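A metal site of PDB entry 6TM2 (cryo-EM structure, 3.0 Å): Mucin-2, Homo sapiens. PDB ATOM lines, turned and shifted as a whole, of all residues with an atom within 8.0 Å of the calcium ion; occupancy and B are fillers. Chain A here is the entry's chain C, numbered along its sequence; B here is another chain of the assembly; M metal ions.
OD1 of Asp 123 is in hydrogen-bond range of N of His 248, at 3.0 Å. The backbone carbonyl oxygen (O) of Asn 245 lies close to the backbone NH (N) of Gly 237 (3.3 Å). The guanidinium group (NE) of Arg 249 sits at hydrogen-bond distance from the side-chain amide oxygen (OD1) of Asn 251, 2.6 Å away. OD2 of Asp 253 lies within hydrogen-bond range of OG1 of Thr 121, at 2.9 Å. The backbone carbonyl oxygen (O) of Asn 252 is in hydrogen-bond range of the side-chain hydroxyl (OG1) of Thr 255 (2.8 Å).
OD2 of Asp 123 binds the calcium ion (2.2 Å). The calcium ion is bound by the side-chain amide oxygen (OD1) of Asn 245 (2.4 Å). O of Arg 249 is bound to the calcium ion (2.5 Å). The side-chain carboxylate (OD1) of Asp 253 is bound to the calcium ion. OD1 of Asp 247 is bound to the calcium ion, 2.5 Å away. OD1 of Asn 252 binds the calcium ion, 2.8 Å away.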
ATOM      1  N   THR A 121      10.615 -23.803 -16.516  1.00  0.00           N
ATOM      2  CA  THR A 121      10.836 -25.204 -16.837  1.00  0.00           C
ATOM      3  C   THR A 121      11.191 -25.363 -18.315  1.00  0.00           C
ATOM      4  O   THR A 121      11.171 -24.398 -19.084  1.00  0.00           O
ATOM      5  CB  THR A 121       9.609 -26.044 -16.481  1.00  0.00           C
ATOM      6  OG1 THR A 121       8.505 -25.653 -17.292  1.00  0.00           O
ATOM      7  CG2 THR A 121       9.235 -25.822 -15.037  1.00  0.00           C
ATOM      8  N   PHE A 122      11.554 -26.588 -18.708  1.00  0.00           N
ATOM      9  CA  PHE A 122      11.885 -26.893 -20.105  1.00  0.00           C
ATOM     10  C   PHE A 122      10.726 -26.614 -21.064  1.00  0.00           C
ATOM     11  O   PHE A 122      10.974 -26.416 -22.254  1.00  0.00           O
ATOM     12  CB  PHE A 122      12.279 -28.365 -20.291  1.00  0.00           C
ATOM     13  CG  PHE A 122      13.634 -28.726 -19.764  1.00  0.00           C
ATOM     14  CD1 PHE A 122      14.767 -28.431 -20.477  1.00  0.00           C
ATOM     15  CD2 PHE A 122      13.777 -29.459 -18.610  1.00  0.00           C
ATOM     16  CE1 PHE A 122      16.011 -28.783 -20.026  1.00  0.00           C
ATOM     17  CE2 PHE A 122      15.021 -29.805 -18.146  1.00  0.00           C
ATOM     18  CZ  PHE A 122      16.138 -29.467 -18.854  1.00  0.00           C
ATOM     19  N   ASP A 123       9.489 -26.643 -20.576  1.00  0.00           N
ATOM     20  CA  ASP A 123       8.302 -26.359 -21.363  1.00  0.00           C
ATOM     21  C   ASP A 123       7.776 -24.950 -21.149  1.00  0.00           C
ATOM     22  O   ASP A 123       6.721 -24.604 -21.666  1.00  0.00           O
ATOM     23  CB  ASP A 123       7.212 -27.373 -21.030  1.00  0.00           C
ATOM     24  CG  ASP A 123       7.566 -28.757 -21.513  1.00  0.00           C
ATOM     25  OD1 ASP A 123       8.283 -28.872 -22.520  1.00  0.00           O
ATOM     26  OD2 ASP A 123       7.119 -29.730 -20.881  1.00  0.00           O
ATOM     27  N   GLY A 124       8.498 -24.128 -20.390  1.00  0.00           N
ATOM     28  CA  GLY A 124       8.205 -22.719 -20.297  1.00  0.00           C
ATOM     29  C   GLY A 124       7.156 -22.330 -19.298  1.00  0.00           C
ATOM     30  O   GLY A 124       6.251 -21.562 -19.620  1.00  0.00           O
ATOM     31  N   LYS A 125       7.272 -22.816 -18.061  1.00  0.00           N
ATOM     32  CA  LYS A 125       6.314 -22.510 -17.010  1.00  0.00           C
ATOM     33  C   LYS A 125       7.055 -21.777 -15.895  1.00  0.00           C
ATOM     34  O   LYS A 125       8.029 -22.302 -15.347  1.00  0.00           O
ATOM     35  CB  LYS A 125       5.672 -23.787 -16.493  1.00  0.00           C
ATOM     36  CG  LYS A 125       4.585 -23.575 -15.494  1.00  0.00           C
ATOM     37  CD  LYS A 125       3.893 -24.866 -15.201  1.00  0.00           C
ATOM     38  CE  LYS A 125       2.708 -24.635 -14.305  1.00  0.00           C
ATOM     39  NZ  LYS A 125       1.971 -25.909 -14.113  1.00  0.00           N
ATOM     40  N   GLY A 237      10.802 -36.136 -22.797  1.00  0.00           N
ATOM     41  CA  GLY A 237       9.909 -36.959 -22.022  1.00  0.00           C
ATOM     42  C   GLY A 237      10.574 -37.990 -21.147  1.00  0.00           C
ATOM     43  O   GLY A 237       9.916 -38.937 -20.724  1.00  0.00           O
ATOM     44  N   VAL A 239      12.898 -37.012 -18.434  1.00  0.00           N
ATOM     45  CA  VAL A 239      13.485 -36.380 -17.261  1.00  0.00           C
ATOM     46  C   VAL A 239      12.375 -35.983 -16.298  1.00  0.00           C
ATOM     47  O   VAL A 239      11.190 -36.077 -16.606  1.00  0.00           O
ATOM     48  CB  VAL A 239      14.378 -35.170 -17.604  1.00  0.00           C
ATOM     49  CG1 VAL A 239      15.607 -35.603 -18.357  1.00  0.00           C
ATOM     50  CG2 VAL A 239      13.627 -34.133 -18.394  1.00  0.00           C
ATOM     51  N   CYS A 243      12.504 -28.929 -12.964  1.00  0.00           N
ATOM     52  CA  CYS A 243      12.531 -28.350 -14.294  1.00  0.00           C
ATOM     53  C   CYS A 243      11.518 -28.982 -15.232  1.00  0.00           C
ATOM     54  O   CYS A 243      11.528 -28.673 -16.423  1.00  0.00           O
ATOM     55  CB  CYS A 243      13.913 -28.473 -14.913  1.00  0.00           C
ATOM     56  SG  CYS A 243      15.203 -27.472 -14.188  1.00  0.00           S
ATOM     57  N   GLY A 244      10.663 -29.865 -14.744  1.00  0.00           N
ATOM     58  CA  GLY A 244       9.674 -30.482 -15.596  1.00  0.00           C
ATOM     59  C   GLY A 244      10.181 -31.723 -16.275  1.00  0.00           C
ATOM     60  O   GLY A 244      11.197 -32.304 -15.894  1.00  0.00           O
ATOM     61  N   ASN A 245       9.471 -32.130 -17.329  1.00  0.00           N
ATOM     62  CA  ASN A 245       9.770 -33.373 -18.023  1.00  0.00           C
ATOM     63  C   ASN A 245      10.020 -33.280 -19.522  1.00  0.00           C
ATOM     64  O   ASN A 245      10.244 -34.324 -20.138  1.00  0.00           O
ATOM     65  CB  ASN A 245       8.660 -34.405 -17.760  1.00  0.00           C
ATOM     66  CG  ASN A 245       7.285 -33.910 -18.121  1.00  0.00           C
ATOM     67  OD1 ASN A 245       7.104 -32.831 -18.645  1.00  0.00           O
ATOM     68  ND2 ASN A 245       6.288 -34.723 -17.819  1.00  0.00           N
ATOM     69  N   PHE A 246       9.983 -32.084 -20.110  1.00  0.00           N
ATOM     70  CA  PHE A 246      10.495 -31.777 -21.448  1.00  0.00           C
ATOM     71  C   PHE A 246       9.776 -32.595 -22.529  1.00  0.00           C
ATOM     72  O   PHE A 246      10.370 -33.321 -23.327  1.00  0.00           O
ATOM     73  CB  PHE A 246      12.033 -31.940 -21.450  1.00  0.00           C
ATOM     74  CG  PHE A 246      12.730 -31.577 -22.735  1.00  0.00           C
ATOM     75  CD1 PHE A 246      12.653 -30.308 -23.270  1.00  0.00           C
ATOM     76  CD2 PHE A 246      13.626 -32.452 -23.301  1.00  0.00           C
ATOM     77  CE1 PHE A 246      13.328 -29.993 -24.422  1.00  0.00           C
ATOM     78  CE2 PHE A 246      14.330 -32.125 -24.441  1.00  0.00           C
ATOM     79  CZ  PHE A 246      14.171 -30.906 -24.997  1.00  0.00           C
ATOM     80  N   ASP A 247       8.445 -32.467 -22.542  1.00  0.00           N
ATOM     81  CA  ASP A 247       7.632 -33.126 -23.553  1.00  0.00           C
ATOM     82  C   ASP A 247       6.717 -32.181 -24.305  1.00  0.00           C
ATOM     83  O   ASP A 247       5.700 -32.629 -24.837  1.00  0.00           O
ATOM     84  CB  ASP A 247       6.830 -34.285 -22.960  1.00  0.00           C
ATOM     85  CG  ASP A 247       5.898 -33.860 -21.849  1.00  0.00           C
ATOM     86  OD1 ASP A 247       5.946 -32.703 -21.412  1.00  0.00           O
ATOM     87  OD2 ASP A 247       5.100 -34.703 -21.413  1.00  0.00           O
ATOM     88  N   HIS A 248       7.051 -30.883 -24.332  1.00  0.00           N
ATOM     89  CA  HIS A 248       6.364 -29.861 -25.136  1.00  0.00           C
ATOM     90  C   HIS A 248       4.876 -29.777 -24.803  1.00  0.00           C
ATOM     91  O   HIS A 248       4.038 -29.688 -25.688  1.00  0.00           O
ATOM     92  CB  HIS A 248       6.588 -30.098 -26.626  1.00  0.00           C
ATOM     93  CG  HIS A 248       8.034 -30.234 -26.986  1.00  0.00           C
ATOM     94  ND1 HIS A 248       8.869 -29.147 -27.144  1.00  0.00           N
ATOM     95  CD2 HIS A 248       8.799 -31.330 -27.216  1.00  0.00           C
ATOM     96  CE1 HIS A 248      10.082 -29.566 -27.454  1.00  0.00           C
ATOM     97  NE2 HIS A 248      10.069 -30.883 -27.489  1.00  0.00           N
ATOM     98  N   ARG A 249       4.568 -29.808 -23.514  1.00  0.00           N
ATOM     99  CA  ARG A 249       3.198 -29.818 -23.017  1.00  0.00           C
ATOM    100  C   ARG A 249       3.309 -29.413 -21.558  1.00  0.00           C
ATOM    101  O   ARG A 249       3.830 -30.190 -20.760  1.00  0.00           O
ATOM    102  CB  ARG A 249       2.590 -31.204 -23.224  1.00  0.00           C
ATOM    103  CG  ARG A 249       1.180 -31.482 -22.788  1.00  0.00           C
ATOM    104  CD  ARG A 249       1.239 -32.171 -21.464  1.00  0.00           C
ATOM    105  NE  ARG A 249      -0.036 -32.621 -20.923  1.00  0.00           N
ATOM    106  CZ  ARG A 249      -0.531 -33.837 -21.111  1.00  0.00           C
ATOM    107  NH1 ARG A 249       0.143 -34.721 -21.834  1.00  0.00           N
ATOM    108  NH2 ARG A 249      -1.690 -34.171 -20.566  1.00  0.00           N
ATOM    109  N   SER A 250       2.843 -28.220 -21.202  1.00  0.00           N
ATOM    110  CA  SER A 250       3.247 -27.638 -19.925  1.00  0.00           C
ATOM    111  C   SER A 250       2.220 -27.787 -18.823  1.00  0.00           C
ATOM    112  O   SER A 250       2.436 -27.255 -17.732  1.00  0.00           O
ATOM    113  CB  SER A 250       3.563 -26.164 -20.077  1.00  0.00           C
ATOM    114  OG  SER A 250       2.383 -25.423 -20.277  1.00  0.00           O
ATOM    115  N   ASN A 251       1.101 -28.476 -19.050  1.00  0.00           N
ATOM    116  CA  ASN A 251       0.154 -28.655 -17.963  1.00  0.00           C
ATOM    117  C   ASN A 251       0.366 -29.955 -17.204  1.00  0.00           C
ATOM    118  O   ASN A 251      -0.565 -30.456 -16.568  1.00  0.00           O
ATOM    119  CB  ASN A 251      -1.291 -28.530 -18.461  1.00  0.00           C
ATOM    120  CG  ASN A 251      -1.675 -29.552 -19.522  1.00  0.00           C
ATOM    121  OD1 ASN A 251      -0.906 -30.413 -19.893  1.00  0.00           O
ATOM    122  ND2 ASN A 251      -2.910 -29.450 -19.979  1.00  0.00           N
ATOM    123  N   ASN A 252       1.574 -30.502 -17.272  1.00  0.00           N
ATOM    124  CA  ASN A 252       1.952 -31.616 -16.420  1.00  0.00           C
ATOM    125  C   ASN A 252       3.338 -31.431 -15.821  1.00  0.00           C
ATOM    126  O   ASN A 252       3.927 -32.401 -15.339  1.00  0.00           O
ATOM    127  CB  ASN A 252       1.842 -32.964 -17.149  1.00  0.00           C
ATOM    128  CG  ASN A 252       2.697 -33.051 -18.391  1.00  0.00           C
ATOM    129  OD1 ASN A 252       3.440 -32.141 -18.734  1.00  0.00           O
ATOM    130  ND2 ASN A 252       2.613 -34.180 -19.062  1.00  0.00           N
ATOM    131  N   ASP A 253       3.887 -30.217 -15.837  1.00  0.00           N
ATOM    132  CA  ASP A 253       5.190 -29.976 -15.248  1.00  0.00           C
ATOM    133  C   ASP A 253       5.172 -30.047 -13.725  1.00  0.00           C
ATOM    134  O   ASP A 253       6.231 -30.227 -13.123  1.00  0.00           O
ATOM    135  CB  ASP A 253       5.765 -28.639 -15.670  1.00  0.00           C
ATOM    136  CG  ASP A 253       6.253 -28.634 -17.086  1.00  0.00           C
ATOM    137  OD1 ASP A 253       6.597 -29.706 -17.595  1.00  0.00           O
ATOM    138  OD2 ASP A 253       6.355 -27.546 -17.663  1.00  0.00           O
ATOM    139  N   PHE A 254       4.006 -29.892 -13.095  1.00  0.00           N
ATOM    140  CA  PHE A 254       3.941 -30.065 -11.648  1.00  0.00           C
ATOM    141  C   PHE A 254       3.596 -31.504 -11.283  1.00  0.00           C
ATOM    142  O   PHE A 254       2.672 -31.763 -10.537  1.00  0.00           O
ATOM    143  CB  PHE A 254       2.947 -29.101 -11.023  1.00  0.00           C
ATOM    144  CG  PHE A 254       3.391 -27.650 -11.008  1.00  0.00           C
ATOM    145  CD1 PHE A 254       4.659 -27.286 -11.408  1.00  0.00           C
ATOM    146  CD2 PHE A 254       2.566 -26.687 -10.490  1.00  0.00           C
ATOM    147  CE1 PHE A 254       5.057 -25.993 -11.370  1.00  0.00           C
ATOM    148  CE2 PHE A 254       2.977 -25.368 -10.439  1.00  0.00           C
ATOM    149  CZ  PHE A 254       4.222 -25.033 -10.874  1.00  0.00           C
ATOM    150  N   THR A 255       4.381 -32.439 -11.791  1.00  0.00           N
ATOM    151  CA  THR A 255       4.319 -33.835 -11.370  1.00  0.00           C
ATOM    152  C   THR A 255       5.266 -34.021 -10.197  1.00  0.00           C
ATOM    153  O   THR A 255       6.433 -33.648 -10.277  1.00  0.00           O
ATOM    154  CB  THR A 255       4.709 -34.766 -12.513  1.00  0.00           C
ATOM    155  OG1 THR A 255       3.846 -34.564 -13.628  1.00  0.00           O
ATOM    156  CG2 THR A 255       4.586 -36.197 -12.081  1.00  0.00           C
ATOM    157  N   GLY B 513      -2.812 -27.852 -24.398  1.00  0.00           N
ATOM    158  CA  GLY B 513      -2.073 -28.250 -23.225  1.00  0.00           C
ATOM    159  C   GLY B 513      -0.875 -27.385 -22.914  1.00  0.00           C
ATOM    160  O   GLY B 513      -0.592 -27.132 -21.746  1.00  0.00           O
ATOM    161  N   LEU B 514      -0.155 -26.933 -23.936  1.00  0.00           N
ATOM    162  CA  LEU B 514       0.965 -26.011 -23.788  1.00  0.00           C
ATOM    163  C   LEU B 514       0.450 -24.579 -23.835  1.00  0.00           C
ATOM    164  O   LEU B 514      -0.465 -24.269 -24.591  1.00  0.00           O
ATOM    165  CB  LEU B 514       1.977 -26.246 -24.904  1.00  0.00           C
ATOM    166  CG  LEU B 514       3.269 -25.443 -25.029  1.00  0.00           C
ATOM    167  CD1 LEU B 514       4.222 -25.694 -23.899  1.00  0.00           C
ATOM    168  CD2 LEU B 514       3.906 -25.795 -26.349  1.00  0.00           C
HETATM  169 CA    CA M   1       5.814 -31.012 -19.572  1.00  0.00          CA
